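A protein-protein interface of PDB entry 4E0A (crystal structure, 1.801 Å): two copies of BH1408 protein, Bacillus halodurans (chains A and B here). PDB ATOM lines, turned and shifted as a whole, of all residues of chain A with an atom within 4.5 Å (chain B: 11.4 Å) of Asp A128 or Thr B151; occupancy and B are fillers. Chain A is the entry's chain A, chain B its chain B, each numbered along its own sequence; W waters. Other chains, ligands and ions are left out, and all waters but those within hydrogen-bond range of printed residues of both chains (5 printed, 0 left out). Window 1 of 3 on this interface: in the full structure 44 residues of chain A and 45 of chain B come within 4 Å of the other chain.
Of the 9 printed residues of chain A, 8 touch a printed residue of chain B. Hydrophobic or aromatic side chains of chain A that line the printed part of chain B: Leu A127, Val A129 and Tyr A130. Among the printed residues, no Asp or Glu carboxylate lies within 4 Å of a Lys or Arg side-chain nitrogen of the other chain.
Water W3 lies within hydrogen-bond range of the side-chain carboxylate of Glu B153 (2.6 Å), the backbone carbonyl oxygen of Cys A147 (3.1 Å) and the guanidinium group of Arg B29 (3.4 Å). Water W1 lies within hydrogen-bond range of the side-chain hydroxyl (OH) of Tyr A130 (2.6 Å) and the side-chain amide oxygen (OE1) of Gln B148 (3.3 Å). Water W2 lies within hydrogen-bond range of OH of Tyr B130 (2.6 Å) and OE1 of Gln A148 (3.1 Å). Water W4 lies within hydrogen-bond range of O of Cys A147 (2.8 Å) and OD2 of Asp B131 (2.8 Å). Water W5 lies within hydrogen-bond range of the backbone carbonyl oxygen of Gln A148 (3.0 Å), the backbone NH of Asp B131 (3.3 Å) and the backbone NH of Phe B132 (3.4 Å).
O of Leu A127 lies within hydrogen-bond range of N of Met B152 (2.8 Å). The side-chain carboxylate (OD2) of Asp A128 is in hydrogen-bond range of the side-chain hydroxyl (OG1) of Thr B151, at 2.7 Å. The backbone carbonyl oxygen (O) of Val A129 sits at hydrogen-bond distance from the backbone NH (N) of Gln B150, at 2.8 Å. The backbone carbonyl oxygen of Arg A146 sits at hydrogen-bond distance from the backbone NH of Glu B153, 2.8 Å away. The side-chain carboxylate (OD1) of Asp B131 is in hydrogen-bond range of the side-chain sulfur (SG) of Cys A147, at 3.8 Å. The backbone carbonyl oxygen of Gln A148 lies within hydrogen-bond range of the backbone NH of Asp B131 (2.9 Å). The backbone NH (N) of Gln A148 is in hydrogen-bond range of the backbone carbonyl oxygen (O) of Thr B151 (2.8 Å). OE1 of Glu B153 lies within hydrogen-bond range of NE2 of Gln A148, at 2.9 Å. The backbone NH (N) of Thr B151 lies within hydrogen-bond range of the backbone carbonyl oxygen (O) of Lys A149, at 2.8 Å.
Among the printed residues, merely in contact across the chains: Leu A127 with Gln B150 (3.8 Å), Leu A127 with Thr B151 (3.3 Å), Asp A128 with Gln B150 (3.3 Å), Val A129 with Lys B149 (3.3 Å), Val A129 with Met B152 (3.8 Å), Tyr A130 with Gln B148 (3.5 Å), Tyr A130 with Lys B149 (3.7 Å), Arg A146 with Met B152 (3.3 Å), Arg A146 with Pro B155 (3.5 Å), Cys A147 with Gln B150 (3.6 Å), Cys A147 with Thr B151 (3.7 Å), Gln A148 with Arg B29 (3.9 Å), Gln A148 with Ile B32 (3.9 Å), Gln A148 with Tyr B130 (3.6 Å), Lys A149 with Val B129 (3.2 Å), Lys A149 with Tyr B130 (3.7 Å), Lys A149 with Asp B131 (3.9 Å) and Lys A149 with Gln B150 (3.5 Å).
OD1 of Asp A128 sits at hydrogen-bond distance from OH of Tyr A90, at 2.4 Å. The side-chain sulfur (SG) of Cys A147 lies within hydrogen-bond range of the backbone carbonyl oxygen (O) of Lys A149. The side-chain carboxylate of Asp B31 is in salt-bridge range of the guanidinium group of Arg B29 (2.9 Å). The side-chain carboxylate (OE2) of Glu B153 is in salt-bridge range of the guanidinium group (NH1) of Arg B29 (2.8 Å). SG of Cys B147 is in hydrogen-bond range of O of Lys B149. The side-chain sulfur (SD) of Met B152 sits close to the side-chain amide oxygen (OE1) of Gln B150 (3.1 Å).
Of chain B, only Gln B150 and Thr B151 come within 4 Å of Asp A128. Of the printed residues of chain B, Tyr A130 touches Gln B148 and Lys B149. Of chain B, only Val B129 (3.2 Å), Tyr B130 (3.7 Å), Asp B131 (3.9 Å), Gln B150 (3.5 Å) and Thr B151 (2.8 Å) come within 4 Å of Lys A149. Of the printed residues of chain A, Val B129 touches Lys A149 (3.2 Å). Of the printed residues of chain A, Tyr B130 touches Gln A148 and Lys A149. Thr B151 touches just these residues of chain A: Leu A127 (3.3 Å), Asp A128 (2.7 Å), Cys A147 (3.7 Å), Gln A148 (2.8 Å) and Lys A149 (2.8 Å). The nearest printed residue of chain A that does not touch Ile B32 is Lys A149 (7.1 Å).
Val A129 touches Lys B149, and with the chains exchanged Lys A149 touches Val B129. Tyr A130 touches Gln B148, and with the chains exchanged Gln A148 touches Tyr B130. Tyr A130 touches Lys B149, and with the chains exchanged Lys A149 touches Tyr B130. Positions printed for both chains: 90, 127, 128, 129, 130, 147, 148 and 149.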
ATOM      1  N   TYR A  90      -8.015 -14.258 -21.264  1.00  0.00           N
ATOM      2  CA  TYR A  90      -9.154 -15.034 -21.733  1.00  0.00           C
ATOM      3  C   TYR A  90      -9.612 -15.985 -20.643  1.00  0.00           C
ATOM      4  O   TYR A  90      -8.832 -16.815 -20.154  1.00  0.00           O
ATOM      5  CB  TYR A  90      -8.808 -15.826 -22.982  1.00  0.00           C
ATOM      6  CG  TYR A  90      -9.988 -16.589 -23.544  1.00  0.00           C
ATOM      7  CD1 TYR A  90     -10.988 -15.930 -24.249  1.00  0.00           C
ATOM      8  CD2 TYR A  90     -10.116 -17.970 -23.358  1.00  0.00           C
ATOM      9  CE1 TYR A  90     -12.079 -16.626 -24.774  1.00  0.00           C
ATOM     10  CE2 TYR A  90     -11.213 -18.664 -23.867  1.00  0.00           C
ATOM     11  CZ  TYR A  90     -12.181 -17.983 -24.582  1.00  0.00           C
ATOM     12  OH  TYR A  90     -13.268 -18.663 -25.103  1.00  0.00           O
ATOM     13  N   LEU A 127     -14.151 -13.629 -22.938  1.00  0.00           N
ATOM     14  CA  LEU A 127     -14.618 -14.995 -22.701  1.00  0.00           C
ATOM     15  C   LEU A 127     -15.673 -15.324 -23.728  1.00  0.00           C
ATOM     16  O   LEU A 127     -16.170 -14.429 -24.413  1.00  0.00           O
ATOM     17  CB  LEU A 127     -15.195 -15.146 -21.284  1.00  0.00           C
ATOM     18  CG  LEU A 127     -16.408 -14.294 -20.895  1.00  0.00           C
ATOM     19  CD1 LEU A 127     -17.758 -14.861 -21.398  1.00  0.00           C
ATOM     20  CD2 LEU A 127     -16.426 -14.135 -19.387  1.00  0.00           C
ATOM     21  N   ASP A 128     -16.052 -16.596 -23.815  1.00  0.00           N
ATOM     22  CA  ASP A 128     -17.158 -16.971 -24.677  1.00  0.00           C
ATOM     23  C   ASP A 128     -18.270 -17.600 -23.879  1.00  0.00           C
ATOM     24  O   ASP A 128     -18.031 -18.406 -22.991  1.00  0.00           O
ATOM     25  CB  ASP A 128     -16.704 -17.920 -25.777  1.00  0.00           C
ATOM     26  CG  ASP A 128     -15.812 -17.233 -26.797  1.00  0.00           C
ATOM     27  OD1 ASP A 128     -14.587 -17.477 -26.780  1.00  0.00           O
ATOM     28  OD2 ASP A 128     -16.334 -16.431 -27.603  1.00  0.00           O
ATOM     29  N   VAL A 129     -19.497 -17.229 -24.211  1.00  0.00           N
ATOM     30  CA  VAL A 129     -20.642 -17.802 -23.527  1.00  0.00           C
ATOM     31  C   VAL A 129     -21.701 -18.258 -24.544  1.00  0.00           C
ATOM     32  O   VAL A 129     -21.938 -17.596 -25.563  1.00  0.00           O
ATOM     33  CB  VAL A 129     -21.223 -16.800 -22.500  1.00  0.00           C
ATOM     34  CG1 VAL A 129     -21.732 -15.545 -23.211  1.00  0.00           C
ATOM     35  CG2 VAL A 129     -22.318 -17.463 -21.673  1.00  0.00           C
ATOM     36  N   TYR A 130     -22.329 -19.392 -24.265  1.00  0.00           N
ATOM     37  CA  TYR A 130     -23.369 -19.914 -25.153  1.00  0.00           C
ATOM     38  C   TYR A 130     -24.692 -19.178 -25.014  1.00  0.00           C
ATOM     39  O   TYR A 130     -25.067 -18.757 -23.918  1.00  0.00           O
ATOM     40  CB  TYR A 130     -23.528 -21.430 -24.985  1.00  0.00           C
ATOM     41  CG  TYR A 130     -22.461 -22.147 -25.760  1.00  0.00           C
ATOM     42  CD1 TYR A 130     -21.182 -22.274 -25.247  1.00  0.00           C
ATOM     43  CD2 TYR A 130     -22.711 -22.617 -27.048  1.00  0.00           C
ATOM     44  CE1 TYR A 130     -20.190 -22.885 -25.962  1.00  0.00           C
ATOM     45  CE2 TYR A 130     -21.721 -23.240 -27.776  1.00  0.00           C
ATOM     46  CZ  TYR A 130     -20.456 -23.368 -27.224  1.00  0.00           C
ATOM     47  OH  TYR A 130     -19.443 -23.985 -27.926  1.00  0.00           O
ATOM     48  N   ARG A 146     -19.530  -6.605 -22.263  1.00  0.00           N
ATOM     49  CA  ARG A 146     -20.362  -6.338 -23.434  1.00  0.00           C
ATOM     50  C   ARG A 146     -20.035  -7.318 -24.560  1.00  0.00           C
ATOM     51  O   ARG A 146     -18.948  -7.904 -24.585  1.00  0.00           O
ATOM     52  CB  ARG A 146     -20.178  -4.882 -23.897  1.00  0.00           C
ATOM     53  CG  ARG A 146     -18.797  -4.572 -24.439  1.00  0.00           C
ATOM     54  CD  ARG A 146     -18.376  -3.127 -24.170  1.00  0.00           C
ATOM     55  NE  ARG A 146     -18.118  -2.889 -22.750  1.00  0.00           N
ATOM     56  CZ  ARG A 146     -17.404  -1.870 -22.279  1.00  0.00           C
ATOM     57  NH1 ARG A 146     -16.862  -0.993 -23.115  1.00  0.00           N
ATOM     58  NH2 ARG A 146     -17.223  -1.732 -20.971  1.00  0.00           N
ATOM     59  N   CYS A 147     -20.979  -7.504 -25.481  1.00  0.00           N
ATOM     60  CA  CYS A 147     -20.772  -8.423 -26.598  1.00  0.00           C
ATOM     61  C   CYS A 147     -19.843  -7.812 -27.625  1.00  0.00           C
ATOM     62  O   CYS A 147     -20.066  -6.688 -28.101  1.00  0.00           O
ATOM     63  CB  CYS A 147     -22.100  -8.826 -27.258  1.00  0.00           C
ATOM     64  SG  CYS A 147     -21.905  -9.962 -28.672  1.00  0.00           S
ATOM     65  N   GLN A 148     -18.787  -8.547 -27.951  1.00  0.00           N
ATOM     66  CA  GLN A 148     -17.843  -8.113 -28.965  1.00  0.00           C
ATOM     67  C   GLN A 148     -18.297  -8.613 -30.333  1.00  0.00           C
ATOM     68  O   GLN A 148     -18.392  -7.845 -31.301  1.00  0.00           O
ATOM     69  CB  GLN A 148     -16.468  -8.674 -28.653  1.00  0.00           C
ATOM     70  CG  GLN A 148     -15.386  -8.206 -29.601  1.00  0.00           C
ATOM     71  CD  GLN A 148     -14.104  -8.980 -29.394  1.00  0.00           C
ATOM     72  OE1 GLN A 148     -13.853  -9.986 -30.063  1.00  0.00           O
ATOM     73  NE2 GLN A 148     -13.295  -8.532 -28.448  1.00  0.00           N
ATOM     74  N   LYS A 149     -18.551  -9.914 -30.408  1.00  0.00           N
ATOM     75  CA  LYS A 149     -18.978 -10.557 -31.647  1.00  0.00           C
ATOM     76  C   LYS A 149     -19.717 -11.830 -31.284  1.00  0.00           C
ATOM     77  O   LYS A 149     -19.640 -12.315 -30.148  1.00  0.00           O
ATOM     78  CB  LYS A 149     -17.770 -10.878 -32.543  1.00  0.00           C
ATOM     79  CG  LYS A 149     -16.698 -11.740 -31.868  1.00  0.00           C
ATOM     80  CD  LYS A 149     -15.576 -12.091 -32.848  1.00  0.00           C
ATOM     81  CE  LYS A 149     -14.354 -12.652 -32.135  1.00  0.00           C
ATOM     82  NZ  LYS A 149     -14.603 -14.019 -31.606  1.00  0.00           N
ATOM     83  N   ARG B  29     -14.477  -0.542 -34.915  1.00  0.00           N
ATOM     84  CA  ARG B  29     -13.605  -1.153 -33.909  1.00  0.00           C
ATOM     85  C   ARG B  29     -12.119  -0.997 -34.244  1.00  0.00           C
ATOM     86  O   ARG B  29     -11.426  -1.983 -34.517  1.00  0.00           O
ATOM     87  CB  ARG B  29     -13.945  -2.629 -33.717  1.00  0.00           C
ATOM     88  CG  ARG B  29     -15.313  -2.884 -33.071  1.00  0.00           C
ATOM     89  CD  ARG B  29     -15.425  -2.250 -31.700  1.00  0.00           C
ATOM     90  NE  ARG B  29     -14.401  -2.722 -30.765  1.00  0.00           N
ATOM     91  CZ  ARG B  29     -14.579  -3.713 -29.898  1.00  0.00           C
ATOM     92  NH1 ARG B  29     -15.741  -4.356 -29.850  1.00  0.00           N
ATOM     93  NH2 ARG B  29     -13.596  -4.064 -29.077  1.00  0.00           N
ATOM     94  N   ASP B  31      -9.792  -0.479 -32.353  1.00  0.00           N
ATOM     95  CA  ASP B  31      -8.957  -1.095 -31.332  1.00  0.00           C
ATOM     96  C   ASP B  31      -8.624  -2.524 -31.709  1.00  0.00           C
ATOM     97  O   ASP B  31      -7.704  -3.132 -31.149  1.00  0.00           O
ATOM     98  CB  ASP B  31      -9.633  -1.042 -29.951  1.00  0.00           C
ATOM     99  CG  ASP B  31     -10.993  -1.737 -29.924  1.00  0.00           C
ATOM    100  OD1 ASP B  31     -11.711  -1.719 -30.944  1.00  0.00           O
ATOM    101  OD2 ASP B  31     -11.350  -2.302 -28.867  1.00  0.00           O
ATOM    102  N   ILE B  32      -9.381  -3.073 -32.654  1.00  0.00           N
ATOM    103  CA  ILE B  32      -9.135  -4.436 -33.119  1.00  0.00           C
ATOM    104  C   ILE B  32      -8.617  -4.466 -34.559  1.00  0.00           C
ATOM    105  O   ILE B  32      -7.676  -5.200 -34.876  1.00  0.00           O
ATOM    106  CB  ILE B  32     -10.407  -5.311 -32.974  1.00  0.00           C
ATOM    107  CG1 ILE B  32     -10.742  -5.478 -31.489  1.00  0.00           C
ATOM    108  CG2 ILE B  32     -10.208  -6.665 -33.635  1.00  0.00           C
ATOM    109  CD1 ILE B  32     -12.106  -6.032 -31.220  1.00  0.00           C
ATOM    110  N   PHE B  33      -9.229  -3.654 -35.414  1.00  0.00           N
ATOM    111  CA  PHE B  33      -8.936  -3.645 -36.843  1.00  0.00           C
ATOM    112  C   PHE B  33      -8.051  -2.469 -37.205  1.00  0.00           C
ATOM    113  O   PHE B  33      -8.189  -1.380 -36.646  1.00  0.00           O
ATOM    114  CB  PHE B  33     -10.250  -3.570 -37.627  1.00  0.00           C
ATOM    115  CG  PHE B  33     -11.141  -4.742 -37.394  1.00  0.00           C
ATOM    116  CD1 PHE B  33     -12.077  -4.728 -36.376  1.00  0.00           C
ATOM    117  CD2 PHE B  33     -11.014  -5.873 -38.170  1.00  0.00           C
ATOM    118  CE1 PHE B  33     -12.891  -5.817 -36.155  1.00  0.00           C
ATOM    119  CE2 PHE B  33     -11.822  -6.978 -37.961  1.00  0.00           C
ATOM    120  CZ  PHE B  33     -12.761  -6.953 -36.951  1.00  0.00           C
ATOM    121  N   MET B  83     -16.917 -33.433 -26.312  1.00  0.00           N
ATOM    122  CA  MET B  83     -17.520 -32.718 -27.451  1.00  0.00           C
ATOM    123  C   MET B  83     -17.899 -33.672 -28.581  1.00  0.00           C
ATOM    124  O   MET B  83     -17.132 -34.577 -28.936  1.00  0.00           O
ATOM    125  CB  MET B  83     -16.598 -31.623 -28.015  1.00  0.00           C
ATOM    126  CG  MET B  83     -16.061 -30.626 -26.998  1.00  0.00           C
ATOM    127  SD  MET B  83     -17.428 -29.437 -26.316  1.00  0.00           S
ATOM    128  CE  MET B  83     -17.470 -28.137 -27.772  1.00  0.00           C
ATOM    129  N   TYR B  90     -17.874 -23.206 -42.512  1.00  0.00           N
ATOM    130  CA  TYR B  90     -17.605 -21.930 -41.857  1.00  0.00           C
ATOM    131  C   TYR B  90     -17.362 -20.864 -42.898  1.00  0.00           C
ATOM    132  O   TYR B  90     -16.456 -20.991 -43.726  1.00  0.00           O
ATOM    133  CB  TYR B  90     -16.383 -22.011 -40.945  1.00  0.00           C
ATOM    134  CG  TYR B  90     -16.136 -20.730 -40.177  1.00  0.00           C
ATOM    135  CD1 TYR B  90     -16.882 -20.418 -39.043  1.00  0.00           C
ATOM    136  CD2 TYR B  90     -15.152 -19.828 -40.582  1.00  0.00           C
ATOM    137  CE1 TYR B  90     -16.650 -19.229 -38.333  1.00  0.00           C
ATOM    138  CE2 TYR B  90     -14.917 -18.653 -39.889  1.00  0.00           C
ATOM    139  CZ  TYR B  90     -15.665 -18.355 -38.765  1.00  0.00           C
ATOM    140  OH  TYR B  90     -15.431 -17.179 -38.069  1.00  0.00           O
ATOM    141  N   LEU B 127     -20.712 -18.833 -38.827  1.00  0.00           N
ATOM    142  CA  LEU B 127     -19.916 -17.659 -39.153  1.00  0.00           C
ATOM    143  C   LEU B 127     -19.816 -16.777 -37.913  1.00  0.00           C
ATOM    144  O   LEU B 127     -20.552 -16.967 -36.948  1.00  0.00           O
ATOM    145  CB  LEU B 127     -20.553 -16.898 -40.325  1.00  0.00           C
ATOM    146  CG  LEU B 127     -21.965 -16.311 -40.170  1.00  0.00           C
ATOM    147  CD1 LEU B 127     -21.957 -14.990 -39.400  1.00  0.00           C
ATOM    148  CD2 LEU B 127     -22.621 -16.087 -41.541  1.00  0.00           C
ATOM    149  N   ASP B 128     -18.938 -15.784 -37.951  1.00  0.00           N
ATOM    150  CA  ASP B 128     -18.851 -14.839 -36.848  1.00  0.00           C
ATOM    151  C   ASP B 128     -19.118 -13.412 -37.311  1.00  0.00           C
ATOM    152  O   ASP B 128     -18.621 -12.988 -38.362  1.00  0.00           O
ATOM    153  CB  ASP B 128     -17.487 -14.960 -36.182  1.00  0.00           C
ATOM    154  CG  ASP B 128     -17.372 -16.212 -35.330  1.00  0.00           C
ATOM    155  OD1 ASP B 128     -16.771 -17.205 -35.788  1.00  0.00           O
ATOM    156  OD2 ASP B 128     -17.899 -16.199 -34.200  1.00  0.00           O
ATOM    157  N   VAL B 129     -19.911 -12.672 -36.541  1.00  0.00           N
ATOM    158  CA  VAL B 129     -20.244 -11.304 -36.918  1.00  0.00           C
ATOM    159  C   VAL B 129     -19.996 -10.361 -35.743  1.00  0.00           C
ATOM    160  O   VAL B 129     -20.321 -10.694 -34.603  1.00  0.00           O
ATOM    161  CB  VAL B 129     -21.697 -11.197 -37.429  1.00  0.00           C
ATOM    162  CG1 VAL B 129     -22.642 -11.817 -36.430  1.00  0.00           C
ATOM    163  CG2 VAL B 129     -22.076  -9.741 -37.694  1.00  0.00           C
ATOM    164  N   TYR B 130     -19.392  -9.204 -36.005  1.00  0.00           N
ATOM    165  CA  TYR B 130     -19.162  -8.243 -34.922  1.00  0.00           C
ATOM    166  C   TYR B 130     -20.461  -7.596 -34.469  1.00  0.00           C
ATOM    167  O   TYR B 130     -21.365  -7.377 -35.263  1.00  0.00           O
ATOM    168  CB  TYR B 130     -18.066  -7.222 -35.269  1.00  0.00           C
ATOM    169  CG  TYR B 130     -16.715  -7.862 -35.100  1.00  0.00           C
ATOM    170  CD1 TYR B 130     -16.246  -8.777 -36.030  1.00  0.00           C
ATOM    171  CD2 TYR B 130     -15.946  -7.627 -33.961  1.00  0.00           C
ATOM    172  CE1 TYR B 130     -15.022  -9.411 -35.856  1.00  0.00           C
ATOM    173  CE2 TYR B 130     -14.724  -8.253 -33.780  1.00  0.00           C
ATOM    174  CZ  TYR B 130     -14.267  -9.139 -34.735  1.00  0.00           C
ATOM    175  OH  TYR B 130     -13.053  -9.768 -34.567  1.00  0.00           O
ATOM    176  N   ASP B 131     -20.547  -7.325 -33.173  1.00  0.00           N
ATOM    177  CA  ASP B 131     -21.787  -6.887 -32.547  1.00  0.00           C
ATOM    178  C   ASP B 131     -22.349  -5.595 -33.171  1.00  0.00           C
ATOM    179  O   ASP B 131     -23.565  -5.418 -33.243  1.00  0.00           O
ATOM    180  CB  ASP B 131     -21.551  -6.724 -31.032  1.00  0.00           C
ATOM    181  CG  ASP B 131     -22.770  -6.220 -30.291  1.00  0.00           C
ATOM    182  OD1 ASP B 131     -23.723  -7.012 -30.121  1.00  0.00           O
ATOM    183  OD2 ASP B 131     -22.769  -5.035 -29.865  1.00  0.00           O
ATOM    184  N   PHE B 132     -21.475  -4.701 -33.641  1.00  0.00           N
ATOM    185  CA  PHE B 132     -21.929  -3.418 -34.206  1.00  0.00           C
ATOM    186  C   PHE B 132     -22.635  -3.596 -35.552  1.00  0.00           C
ATOM    187  O   PHE B 132     -23.319  -2.684 -36.026  1.00  0.00           O
ATOM    188  CB  PHE B 132     -20.742  -2.438 -34.393  1.00  0.00           C
ATOM    189  CG  PHE B 132     -19.838  -2.802 -35.556  1.00  0.00           C
ATOM    190  CD1 PHE B 132     -18.736  -3.612 -35.365  1.00  0.00           C
ATOM    191  CD2 PHE B 132     -20.116  -2.355 -36.844  1.00  0.00           C
ATOM    192  CE1 PHE B 132     -17.918  -3.962 -36.426  1.00  0.00           C
ATOM    193  CE2 PHE B 132     -19.312  -2.709 -37.902  1.00  0.00           C
ATOM    194  CZ  PHE B 132     -18.208  -3.517 -37.690  1.00  0.00           C
ATOM    195  N   LYS B 137     -26.241  -8.615 -39.221  1.00  0.00           N
ATOM    196  CA  LYS B 137     -27.118  -9.367 -38.319  1.00  0.00           C
ATOM    197  C   LYS B 137     -28.539  -9.491 -38.884  1.00  0.00           C
ATOM    198  O   LYS B 137     -29.147 -10.555 -38.808  1.00  0.00           O
ATOM    199  CB  LYS B 137     -27.148  -8.750 -36.914  1.00  0.00           C
ATOM    200  CG  LYS B 137     -25.842  -8.980 -36.137  1.00  0.00           C
ATOM    201  CD  LYS B 137     -26.007  -8.789 -34.623  1.00  0.00           C
ATOM    202  CE  LYS B 137     -26.019  -7.326 -34.222  1.00  0.00           C
ATOM    203  NZ  LYS B 137     -25.808  -7.138 -32.746  1.00  0.00           N
ATOM    204  N   CYS B 147     -27.990 -16.931 -33.007  1.00  0.00           N
ATOM    205  CA  CYS B 147     -26.770 -16.901 -32.215  1.00  0.00           C
ATOM    206  C   CYS B 147     -26.536 -18.244 -31.557  1.00  0.00           C
ATOM    207  O   CYS B 147     -27.425 -18.792 -30.902  1.00  0.00           O
ATOM    208  CB  CYS B 147     -26.830 -15.810 -31.146  1.00  0.00           C
ATOM    209  SG  CYS B 147     -25.273 -15.654 -30.248  1.00  0.00           S
ATOM    210  N   GLN B 148     -25.334 -18.774 -31.742  1.00  0.00           N
ATOM    211  CA  GLN B 148     -24.904 -19.980 -31.057  1.00  0.00           C
ATOM    212  C   GLN B 148     -24.217 -19.603 -29.758  1.00  0.00           C
ATOM    213  O   GLN B 148     -24.529 -20.126 -28.686  1.00  0.00           O
ATOM    214  CB  GLN B 148     -23.897 -20.726 -31.921  1.00  0.00           C
ATOM    215  CG  GLN B 148     -23.401 -22.023 -31.286  1.00  0.00           C
ATOM    216  CD  GLN B 148     -22.274 -22.621 -32.081  1.00  0.00           C
ATOM    217  OE1 GLN B 148     -21.104 -22.358 -31.808  1.00  0.00           O
ATOM    218  NE2 GLN B 148     -22.617 -23.406 -33.092  1.00  0.00           N
ATOM    219  N   LYS B 149     -23.239 -18.712 -29.876  1.00  0.00           N
ATOM    220  CA  LYS B 149     -22.472 -18.261 -28.715  1.00  0.00           C
ATOM    221  C   LYS B 149     -21.911 -16.877 -28.986  1.00  0.00           C
ATOM    222  O   LYS B 149     -21.938 -16.401 -30.114  1.00  0.00           O
ATOM    223  CB  LYS B 149     -21.343 -19.246 -28.384  1.00  0.00           C
ATOM    224  CG  LYS B 149     -20.225 -19.329 -29.432  1.00  0.00           C
ATOM    225  CD  LYS B 149     -19.180 -20.376 -29.052  1.00  0.00           C
ATOM    226  CE  LYS B 149     -18.394 -20.826 -30.282  1.00  0.00           C
ATOM    227  NZ  LYS B 149     -17.792 -19.648 -30.985  1.00  0.00           N
ATOM    228  N   GLN B 150     -21.410 -16.211 -27.955  1.00  0.00           N
ATOM    229  CA  GLN B 150     -20.849 -14.884 -28.184  1.00  0.00           C
ATOM    230  C   GLN B 150     -19.598 -14.624 -27.361  1.00  0.00           C
ATOM    231  O   GLN B 150     -19.430 -15.153 -26.251  1.00  0.00           O
ATOM    232  CB  GLN B 150     -21.899 -13.808 -27.934  1.00  0.00           C
ATOM    233  CG  GLN B 150     -22.501 -13.836 -26.557  1.00  0.00           C
ATOM    234  CD  GLN B 150     -23.536 -12.738 -26.369  1.00  0.00           C
ATOM    235  OE1 GLN B 150     -23.314 -11.787 -25.626  1.00  0.00           O
ATOM    236  NE2 GLN B 150     -24.666 -12.860 -27.051  1.00  0.00           N
ATOM    237  N   THR B 151     -18.711 -13.827 -27.938  1.00  0.00           N
ATOM    238  CA  THR B 151     -17.507 -13.397 -27.251  1.00  0.00           C
ATOM    239  C   THR B 151     -17.855 -12.135 -26.509  1.00  0.00           C
ATOM    240  O   THR B 151     -18.374 -11.177 -27.095  1.00  0.00           O
ATOM    241  CB  THR B 151     -16.384 -13.073 -28.244  1.00  0.00           C
ATOM    242  OG1 THR B 151     -16.114 -14.213 -29.067  1.00  0.00           O
ATOM    243  CG2 THR B 151     -15.106 -12.661 -27.495  1.00  0.00           C
ATOM    244  N   MET B 152     -17.564 -12.129 -25.218  1.00  0.00           N
ATOM    245  CA  MET B 152     -17.805 -10.968 -24.386  1.00  0.00           C
ATOM    246  C   MET B 152     -16.499 -10.346 -24.010  1.00  0.00           C
ATOM    247  O   MET B 152     -15.481 -11.039 -23.941  1.00  0.00           O
ATOM    248  CB  MET B 152     -18.541 -11.422 -23.149  1.00  0.00           C
ATOM    249  CG  MET B 152     -19.604 -12.334 -23.584  1.00  0.00           C
ATOM    250  SD  MET B 152     -21.178 -11.281 -23.463  1.00  0.00           S
ATOM    251  CE  MET B 152     -21.403 -12.023 -21.711  1.00  0.00           C
ATOM    252  N   GLU B 153     -16.519  -9.028 -23.792  1.00  0.00           N
ATOM    253  CA  GLU B 153     -15.290  -8.298 -23.523  1.00  0.00           C
ATOM    254  C   GLU B 153     -15.471  -7.257 -22.430  1.00  0.00           C
ATOM    255  O   GLU B 153     -16.550  -6.680 -22.275  1.00  0.00           O
ATOM    256  CB  GLU B 153     -14.782  -7.599 -24.790  1.00  0.00           C
ATOM    257  CG  GLU B 153     -15.765  -6.580 -25.330  1.00  0.00           C
ATOM    258  CD  GLU B 153     -15.371  -5.979 -26.670  1.00  0.00           C
ATOM    259  OE1 GLU B 153     -14.189  -6.086 -27.074  1.00  0.00           O
ATOM    260  OE2 GLU B 153     -16.267  -5.398 -27.321  1.00  0.00           O
ATOM    261  N   LEU B 154     -14.394  -7.023 -21.690  1.00  0.00           N
ATOM    262  CA  LEU B 154     -14.342  -5.947 -20.694  1.00  0.00           C
ATOM    263  C   LEU B 154     -13.034  -5.201 -20.911  1.00  0.00           C
ATOM    264  O   LEU B 154     -11.971  -5.687 -20.535  1.00  0.00           O
ATOM    265  CB  LEU B 154     -14.429  -6.517 -19.272  1.00  0.00           C
ATOM    266  CG  LEU B 154     -14.410  -5.454 -18.172  1.00  0.00           C
ATOM    267  CD1 LEU B 154     -15.600  -4.500 -18.306  1.00  0.00           C
ATOM    268  CD2 LEU B 154     -14.362  -6.098 -16.797  1.00  0.00           C
ATOM    269  N   PRO B 155     -13.093  -4.039 -21.585  1.00  0.00           N
ATOM    270  CA  PRO B 155     -11.857  -3.280 -21.823  1.00  0.00           C
ATOM    271  C   PRO B 155     -11.231  -2.833 -20.504  1.00  0.00           C
ATOM    272  O   PRO B 155     -11.958  -2.424 -19.598  1.00  0.00           O
ATOM    273  CB  PRO B 155     -12.334  -2.071 -22.638  1.00  0.00           C
ATOM    274  CG  PRO B 155     -13.599  -2.541 -23.309  1.00  0.00           C
ATOM    275  CD  PRO B 155     -14.249  -3.467 -22.297  1.00  0.00           C
HETATM  276  O   HOH W   1     -19.198 -24.662 -30.407  1.00  0.00           O
HETATM  277  O   HOH W   2     -11.830 -10.356 -32.321  1.00  0.00           O
HETATM  278  O   HOH W   3     -18.431  -4.119 -27.775  1.00  0.00           O
HETATM  279  O   HOH W   4     -21.963  -4.930 -27.145  1.00  0.00           O
HETATM  280  O   HOH W   5     -18.475  -4.982 -32.073  1.00  0.00           O
